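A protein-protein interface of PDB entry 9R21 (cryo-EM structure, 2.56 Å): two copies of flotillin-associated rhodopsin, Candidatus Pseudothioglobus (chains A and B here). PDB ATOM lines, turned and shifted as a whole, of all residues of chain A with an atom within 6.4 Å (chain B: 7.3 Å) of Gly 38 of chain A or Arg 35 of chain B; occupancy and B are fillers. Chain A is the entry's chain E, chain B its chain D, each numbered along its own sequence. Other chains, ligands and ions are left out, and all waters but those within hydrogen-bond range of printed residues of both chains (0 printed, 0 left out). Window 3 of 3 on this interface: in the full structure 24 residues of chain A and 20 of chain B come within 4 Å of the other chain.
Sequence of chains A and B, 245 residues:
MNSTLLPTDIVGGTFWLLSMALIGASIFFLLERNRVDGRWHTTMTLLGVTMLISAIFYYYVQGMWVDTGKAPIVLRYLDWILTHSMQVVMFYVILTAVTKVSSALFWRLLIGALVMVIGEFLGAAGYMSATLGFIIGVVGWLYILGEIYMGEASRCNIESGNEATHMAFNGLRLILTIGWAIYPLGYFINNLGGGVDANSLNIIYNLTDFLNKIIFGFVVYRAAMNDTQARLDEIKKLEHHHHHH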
ATOM      1  N   ARG A  33      36.075 -27.273 -11.681  1.00  0.00           N
ATOM      2  CA  ARG A  33      34.734 -26.832 -11.319  1.00  0.00           C
ATOM      3  C   ARG A  33      33.683 -27.829 -11.790  1.00  0.00           C
ATOM      4  O   ARG A  33      32.576 -27.864 -11.256  1.00  0.00           O
ATOM      5  CB  ARG A  33      34.537 -25.478 -11.985  1.00  0.00           C
ATOM      6  CG  ARG A  33      33.131 -24.918 -12.044  1.00  0.00           C
ATOM      7  CD  ARG A  33      33.161 -23.543 -12.702  1.00  0.00           C
ATOM      8  NE  ARG A  33      33.868 -23.661 -13.970  1.00  0.00           N
ATOM      9  CZ  ARG A  33      33.354 -23.764 -15.173  1.00  0.00           C
ATOM     10  NH1 ARG A  33      34.165 -24.038 -16.182  1.00  0.00           N
ATOM     11  NH2 ARG A  33      32.066 -23.634 -15.364  1.00  0.00           N
ATOM     12  N   VAL A  36      33.386 -31.334  -9.318  1.00  0.00           N
ATOM     13  CA  VAL A  36      32.788 -31.280  -7.993  1.00  0.00           C
ATOM     14  C   VAL A  36      31.274 -31.351  -8.184  1.00  0.00           C
ATOM     15  O   VAL A  36      30.787 -31.069  -9.279  1.00  0.00           O
ATOM     16  CB  VAL A  36      33.201 -30.019  -7.198  1.00  0.00           C
ATOM     17  CG1 VAL A  36      34.694 -29.990  -6.992  1.00  0.00           C
ATOM     18  CG2 VAL A  36      32.765 -28.698  -7.860  1.00  0.00           C
ATOM     19  N   ASP A  37      30.537 -31.708  -7.127  1.00  0.00           N
ATOM     20  CA  ASP A  37      29.094 -31.608  -7.142  1.00  0.00           C
ATOM     21  C   ASP A  37      28.655 -30.227  -7.610  1.00  0.00           C
ATOM     22  O   ASP A  37      29.430 -29.286  -7.597  1.00  0.00           O
ATOM     23  CB  ASP A  37      28.503 -31.802  -5.765  1.00  0.00           C
ATOM     24  CG  ASP A  37      28.133 -33.227  -5.424  1.00  0.00           C
ATOM     25  OD1 ASP A  37      27.559 -33.417  -4.331  1.00  0.00           O
ATOM     26  OD2 ASP A  37      28.415 -34.125  -6.251  1.00  0.00           O
ATOM     27  N   GLY A  38      27.390 -30.096  -7.996  1.00  0.00           N
ATOM     28  CA  GLY A  38      26.903 -28.826  -8.478  1.00  0.00           C
ATOM     29  C   GLY A  38      26.730 -27.869  -7.325  1.00  0.00           C
ATOM     30  O   GLY A  38      26.770 -26.669  -7.574  1.00  0.00           O
ATOM     31  N   ARG A  39      26.609 -28.404  -6.094  1.00  0.00           N
ATOM     32  CA  ARG A  39      26.455 -27.566  -4.913  1.00  0.00           C
ATOM     33  C   ARG A  39      27.729 -26.767  -4.700  1.00  0.00           C
ATOM     34  O   ARG A  39      27.706 -25.784  -3.975  1.00  0.00           O
ATOM     35  CB  ARG A  39      26.057 -28.373  -3.681  1.00  0.00           C
ATOM     36  CG  ARG A  39      27.207 -29.068  -2.975  1.00  0.00           C
ATOM     37  CD  ARG A  39      26.715 -29.796  -1.785  1.00  0.00           C
ATOM     38  NE  ARG A  39      25.486 -30.537  -2.048  1.00  0.00           N
ATOM     39  CZ  ARG A  39      24.358 -30.416  -1.371  1.00  0.00           C
ATOM     40  NH1 ARG A  39      24.286 -29.703  -0.261  1.00  0.00           N
ATOM     41  NH2 ARG A  39      23.271 -31.014  -1.831  1.00  0.00           N
ATOM     42  N   TRP A  40      28.794 -27.116  -5.418  1.00  0.00           N
ATOM     43  CA  TRP A  40      30.095 -26.529  -5.166  1.00  0.00           C
ATOM     44  C   TRP A  40      30.524 -25.621  -6.293  1.00  0.00           C
ATOM     45  O   TRP A  40      31.547 -24.983  -6.157  1.00  0.00           O
ATOM     46  CB  TRP A  40      31.107 -27.654  -4.921  1.00  0.00           C
ATOM     47  CG  TRP A  40      30.928 -28.284  -3.581  1.00  0.00           C
ATOM     48  CD1 TRP A  40      30.456 -29.523  -3.320  1.00  0.00           C
ATOM     49  CD2 TRP A  40      31.201 -27.679  -2.310  1.00  0.00           C
ATOM     50  NE1 TRP A  40      30.398 -29.726  -1.966  1.00  0.00           N
ATOM     51  CE2 TRP A  40      30.833 -28.616  -1.322  1.00  0.00           C
ATOM     52  CE3 TRP A  40      31.727 -26.448  -1.913  1.00  0.00           C
ATOM     53  CZ2 TRP A  40      30.987 -28.373   0.038  1.00  0.00           C
ATOM     54  CZ3 TRP A  40      31.919 -26.213  -0.562  1.00  0.00           C
ATOM     55  CH2 TRP A  40      31.539 -27.160   0.403  1.00  0.00           C
ATOM     56  N   HIS A  41      29.710 -25.496  -7.324  1.00  0.00           N
ATOM     57  CA  HIS A  41      30.069 -24.812  -8.552  1.00  0.00           C
ATOM     58  C   HIS A  41      30.309 -23.309  -8.390  1.00  0.00           C
ATOM     59  O   HIS A  41      31.221 -22.777  -9.029  1.00  0.00           O
ATOM     60  CB  HIS A  41      28.988 -25.145  -9.591  1.00  0.00           C
ATOM     61  CG  HIS A  41      29.315 -24.661 -10.953  1.00  0.00           C
ATOM     62  ND1 HIS A  41      29.181 -23.324 -11.350  1.00  0.00           N
ATOM     63  CD2 HIS A  41      29.809 -25.338 -11.995  1.00  0.00           C
ATOM     64  CE1 HIS A  41      29.616 -23.182 -12.606  1.00  0.00           C
ATOM     65  NE2 HIS A  41      29.977 -24.405 -13.041  1.00  0.00           N
ATOM     66  N   THR A  42      29.491 -22.625  -7.576  1.00  0.00           N
ATOM     67  CA  THR A  42      29.698 -21.220  -7.287  1.00  0.00           C
ATOM     68  C   THR A  42      30.955 -21.000  -6.478  1.00  0.00           C
ATOM     69  O   THR A  42      31.694 -20.064  -6.780  1.00  0.00           O
ATOM     70  CB  THR A  42      28.502 -20.673  -6.544  1.00  0.00           C
ATOM     71  OG1 THR A  42      27.484 -20.935  -7.509  1.00  0.00           O
ATOM     72  CG2 THR A  42      28.578 -19.172  -6.318  1.00  0.00           C
ATOM     73  N   LEU B  31      30.562 -18.502 -16.589  1.00  0.00           N
ATOM     74  CA  LEU B  31      30.732 -19.861 -16.108  1.00  0.00           C
ATOM     75  C   LEU B  31      29.509 -20.320 -15.335  1.00  0.00           C
ATOM     76  O   LEU B  31      29.181 -21.501 -15.379  1.00  0.00           O
ATOM     77  CB  LEU B  31      32.009 -19.931 -15.309  1.00  0.00           C
ATOM     78  CG  LEU B  31      33.295 -19.762 -16.142  1.00  0.00           C
ATOM     79  CD1 LEU B  31      34.522 -20.106 -15.279  1.00  0.00           C
ATOM     80  CD2 LEU B  31      33.331 -20.553 -17.417  1.00  0.00           C
ATOM     81  N   GLU B  32      28.727 -19.380 -14.831  1.00  0.00           N
ATOM     82  CA  GLU B  32      27.526 -19.705 -14.095  1.00  0.00           C
ATOM     83  C   GLU B  32      26.342 -19.805 -15.062  1.00  0.00           C
ATOM     84  O   GLU B  32      25.215 -20.063 -14.649  1.00  0.00           O
ATOM     85  CB  GLU B  32      27.486 -18.611 -13.019  1.00  0.00           C
ATOM     86  CG  GLU B  32      28.482 -18.821 -11.883  1.00  0.00           C
ATOM     87  CD  GLU B  32      27.969 -19.771 -10.815  1.00  0.00           C
ATOM     88  OE1 GLU B  32      28.226 -21.014 -10.898  1.00  0.00           O
ATOM     89  OE2 GLU B  32      27.305 -19.235  -9.896  1.00  0.00           O
ATOM     90  N   ARG B  33      26.616 -19.643 -16.360  1.00  0.00           N
ATOM     91  CA  ARG B  33      25.631 -19.743 -17.427  1.00  0.00           C
ATOM     92  C   ARG B  33      25.111 -21.164 -17.567  1.00  0.00           C
ATOM     93  O   ARG B  33      24.021 -21.386 -18.083  1.00  0.00           O
ATOM     94  CB  ARG B  33      26.350 -19.316 -18.703  1.00  0.00           C
ATOM     95  CG  ARG B  33      25.547 -19.274 -19.981  1.00  0.00           C
ATOM     96  CD  ARG B  33      26.550 -18.869 -21.077  1.00  0.00           C
ATOM     97  NE  ARG B  33      27.166 -20.164 -21.280  1.00  0.00           N
ATOM     98  CZ  ARG B  33      28.283 -20.504 -21.836  1.00  0.00           C
ATOM     99  NH1 ARG B  33      29.455 -20.513 -21.245  1.00  0.00           N
ATOM    100  NH2 ARG B  33      28.106 -21.308 -22.858  1.00  0.00           N
ATOM    101  N   ASN B  34      25.864 -22.128 -17.042  1.00  0.00           N
ATOM    102  CA  ASN B  34      25.575 -23.522 -17.298  1.00  0.00           C
ATOM    103  C   ASN B  34      24.813 -24.107 -16.119  1.00  0.00           C
ATOM    104  O   ASN B  34      24.253 -25.187 -16.232  1.00  0.00           O
ATOM    105  CB  ASN B  34      26.861 -24.244 -17.673  1.00  0.00           C
ATOM    106  CG  ASN B  34      27.459 -23.709 -18.962  1.00  0.00           C
ATOM    107  OD1 ASN B  34      26.835 -23.808 -20.035  1.00  0.00           O
ATOM    108  ND2 ASN B  34      28.650 -23.117 -18.879  1.00  0.00           N
ATOM    109  N   ARG B  35      24.708 -23.353 -15.036  1.00  0.00           N
ATOM    110  CA  ARG B  35      24.068 -23.837 -13.835  1.00  0.00           C
ATOM    111  C   ARG B  35      22.655 -23.291 -13.694  1.00  0.00           C
ATOM    112  O   ARG B  35      21.930 -23.706 -12.793  1.00  0.00           O
ATOM    113  CB  ARG B  35      24.994 -23.465 -12.668  1.00  0.00           C
ATOM    114  CG  ARG B  35      26.329 -24.164 -12.874  1.00  0.00           C
ATOM    115  CD  ARG B  35      26.256 -25.639 -12.558  1.00  0.00           C
ATOM    116  NE  ARG B  35      25.718 -25.736 -11.193  1.00  0.00           N
ATOM    117  CZ  ARG B  35      25.018 -26.752 -10.744  1.00  0.00           C
ATOM    118  NH1 ARG B  35      25.120 -27.933 -11.345  1.00  0.00           N
ATOM    119  NH2 ARG B  35      24.265 -26.616  -9.658  1.00  0.00           N
ATOM    120  N   VAL B  36      22.277 -22.336 -14.533  1.00  0.00           N
ATOM    121  CA  VAL B  36      20.916 -21.823 -14.534  1.00  0.00           C
ATOM    122  C   VAL B  36      20.126 -22.666 -15.536  1.00  0.00           C
ATOM    123  O   VAL B  36      20.730 -23.309 -16.396  1.00  0.00           O
ATOM    124  CB  VAL B  36      20.845 -20.317 -14.876  1.00  0.00           C
ATOM    125  CG1 VAL B  36      21.607 -19.506 -13.857  1.00  0.00           C
ATOM    126  CG2 VAL B  36      21.375 -19.972 -16.279  1.00  0.00           C
ATOM    127  N   ASP B  37      18.793 -22.648 -15.434  1.00  0.00           N
ATOM    128  CA  ASP B  37      17.948 -23.235 -16.450  1.00  0.00           C
ATOM    129  C   ASP B  37      18.351 -22.751 -17.837  1.00  0.00           C
ATOM    130  O   ASP B  37      19.030 -21.747 -17.976  1.00  0.00           O
ATOM    131  CB  ASP B  37      16.497 -22.845 -16.266  1.00  0.00           C
ATOM    132  CG  ASP B  37      15.687 -23.786 -15.405  1.00  0.00           C
ATOM    133  OD1 ASP B  37      14.468 -23.533 -15.288  1.00  0.00           O
ATOM    134  OD2 ASP B  37      16.280 -24.753 -14.868  1.00  0.00           O
ATOM    135  N   GLY B  38      17.895 -23.442 -18.874  1.00  0.00           N
ATOM    136  CA  GLY B  38      18.244 -23.056 -20.221  1.00  0.00           C
ATOM    137  C   GLY B  38      17.474 -21.822 -20.618  1.00  0.00           C
ATOM    138  O   GLY B  38      17.955 -21.112 -21.493  1.00  0.00           O
ATOM    139  N   HIS B  41      19.826 -18.847 -20.302  1.00  0.00           N
ATOM    140  CA  HIS B  41      21.133 -18.914 -20.932  1.00  0.00           C
ATOM    141  C   HIS B  41      21.493 -17.674 -21.758  1.00  0.00           C
ATOM    142  O   HIS B  41      22.651 -17.249 -21.733  1.00  0.00           O
ATOM    143  CB  HIS B  41      21.203 -20.221 -21.738  1.00  0.00           C
ATOM    144  CG  HIS B  41      22.551 -20.500 -22.295  1.00  0.00           C
ATOM    145  ND1 HIS B  41      23.065 -19.863 -23.431  1.00  0.00           N
ATOM    146  CD2 HIS B  41      23.534 -21.297 -21.835  1.00  0.00           C
ATOM    147  CE1 HIS B  41      24.339 -20.252 -23.635  1.00  0.00           C
ATOM    148  NE2 HIS B  41      24.643 -21.133 -22.681  1.00  0.00           N
ATOM    149  N   TYR B 221      21.814 -11.991 -12.229  1.00  0.00           N
ATOM    150  CA  TYR B 221      22.320 -13.284 -11.846  1.00  0.00           C
ATOM    151  C   TYR B 221      21.481 -13.888 -10.720  1.00  0.00           C
ATOM    152  O   TYR B 221      21.228 -15.079 -10.707  1.00  0.00           O
ATOM    153  CB  TYR B 221      23.794 -13.090 -11.464  1.00  0.00           C
ATOM    154  CG  TYR B 221      24.381 -14.279 -10.711  1.00  0.00           C
ATOM    155  CD1 TYR B 221      24.503 -14.248  -9.326  1.00  0.00           C
ATOM    156  CD2 TYR B 221      24.695 -15.470 -11.359  1.00  0.00           C
ATOM    157  CE1 TYR B 221      25.015 -15.325  -8.621  1.00  0.00           C
ATOM    158  CE2 TYR B 221      25.219 -16.547 -10.666  1.00  0.00           C
ATOM    159  CZ  TYR B 221      25.388 -16.474  -9.293  1.00  0.00           C
ATOM    160  OH  TYR B 221      25.862 -17.543  -8.586  1.00  0.00           O
ATOM    161  N   ALA B 224      18.186 -15.282 -12.206  1.00  0.00           N
ATOM    162  CA  ALA B 224      18.342 -16.503 -12.946  1.00  0.00           C
ATOM    163  C   ALA B 224      18.559 -17.640 -11.962  1.00  0.00           C
ATOM    164  O   ALA B 224      17.998 -18.714 -12.118  1.00  0.00           O
ATOM    165  CB  ALA B 224      19.456 -16.336 -13.936  1.00  0.00           C
ATOM    166  N   MET B 225      19.351 -17.391 -10.930  1.00  0.00           N
ATOM    167  CA  MET B 225      19.635 -18.395  -9.913  1.00  0.00           C
ATOM    168  C   MET B 225      18.366 -18.641  -9.098  1.00  0.00           C
ATOM    169  O   MET B 225      17.870 -19.748  -8.967  1.00  0.00           O
ATOM    170  CB  MET B 225      20.802 -17.940  -9.044  1.00  0.00           C
ATOM    171  CG  MET B 225      22.094 -17.897  -9.833  1.00  0.00           C
ATOM    172  SD  MET B 225      22.846 -19.470 -10.327  1.00  0.00           S
ATOM    173  CE  MET B 225      23.382 -19.997  -8.699  1.00  0.00           C
ATOM    174  N   THR B 228      15.921 -20.681 -11.275  1.00  0.00           N
ATOM    175  CA  THR B 228      16.370 -22.020 -11.597  1.00  0.00           C
ATOM    176  C   THR B 228      16.023 -22.949 -10.454  1.00  0.00           C
ATOM    177  O   THR B 228      15.519 -24.035 -10.714  1.00  0.00           O
ATOM    178  CB  THR B 228      17.854 -22.026 -11.877  1.00  0.00           C
ATOM    179  OG1 THR B 228      18.025 -21.067 -12.904  1.00  0.00           O
ATOM    180  CG2 THR B 228      18.310 -23.374 -12.384  1.00  0.00           C
ATOM    181  N   GLN B 229      16.230 -22.448  -9.236  1.00  0.00           N
ATOM    182  CA  GLN B 229      16.050 -23.172  -7.999  1.00  0.00           C
ATOM    183  C   GLN B 229      14.586 -23.351  -7.649  1.00  0.00           C
ATOM    184  O   GLN B 229      14.235 -24.353  -7.054  1.00  0.00           O
ATOM    185  CB  GLN B 229      16.669 -22.332  -6.890  1.00  0.00           C
ATOM    186  CG  GLN B 229      16.725 -23.006  -5.522  1.00  0.00           C
ATOM    187  CD  GLN B 229      17.431 -24.344  -5.552  1.00  0.00           C
ATOM    188  OE1 GLN B 229      18.453 -24.520  -6.230  1.00  0.00           O
ATOM    189  NE2 GLN B 229      16.863 -25.315  -4.850  1.00  0.00           N
ATOM    190  N   LEU B 232      13.322 -26.201  -9.447  1.00  0.00           N
ATOM    191  CA  LEU B 232      13.822 -27.457  -8.926  1.00  0.00           C
ATOM    192  C   LEU B 232      13.042 -27.811  -7.669  1.00  0.00           C
ATOM    193  O   LEU B 232      12.696 -28.971  -7.462  1.00  0.00           O
ATOM    194  CB  LEU B 232      15.316 -27.346  -8.641  1.00  0.00           C
ATOM    195  CG  LEU B 232      16.207 -27.419  -9.880  1.00  0.00           C
ATOM    196  CD1 LEU B 232      17.586 -26.886  -9.592  1.00  0.00           C
ATOM    197  CD2 LEU B 232      16.285 -28.848 -10.380  1.00  0.00           C
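Of chain B, only Arg 35 comes within 4 Å of Gly 38 of chain A.
Arg 35 of chain B touches just these residues of chain A: Gly 38 and His 41.
Printed residues of chain A within 4 Å of Glu 32 of chain B: His 41 and Thr 42.
Of the printed residues of chain B, Thr 42 of chain A touches Glu 32 and Tyr 221.
Printed residues of chain B within 4 Å of His 41 of chain A: Leu 31, Glu 32 and Arg 35.
The nearest residue of chain A that does not touch Arg 35 of chain B is Arg 39 of chain A (4.6 Å).
The nearest printed residue of chain B that does not touch Thr 42 of chain A is Met 225 of chain B (4.4 Å).
O of Leu 31 of chain B touches NH2 of Arg 33 of chain A (3.6 Å).
O of Leu 31 of chain B touches CE1 of His 41 of chain A, at 3.3 Å.
His 41 of chain A touches Arg 35 of chain B (ND1 to CG, 3.3 Å).
CG2 of Thr 42 of chain A touches OH of Tyr 221 of chain B, at 3.9 Å.
OE2 of Glu 32 of chain B is in hydrogen-bond range of OH of Tyr 221 of chain B (2.6 Å).
NH2 of Arg 33 of chain A lies within hydrogen-bond range of NE2 of His 41 of chain A.
5 positions are printed for both chains.
Of the 7 pairs that touch across the chains among the printed residues, none has its exchanged pair printed and touching as well.
Hydrophobic or aromatic side chains of chain A that line the printed part of chain B: His 41.
Of the 15 printed residues of chain B, 4 touch a printed residue of chain A.
Hydrophobic or aromatic side chains of chain B within 4 Å of the printed part of chain A: Leu 31 and Tyr 221.
A ring nitrogen (ND1) of His 41 of chain A sits at hydrogen-bond distance from the side-chain carboxylate (OE1) of Glu 32 of chain B, 2.5 Å away.
The side-chain hydroxyl (OG1) of Thr 42 of chain A lies within hydrogen-bond range of the side-chain carboxylate (OE2) of Glu 32 of chain B.
The backbone carbonyl oxygen of Gly 38 of chain A sits at hydrogen-bond distance from the guanidinium group of Arg 35 of chain B (3.3 Å).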
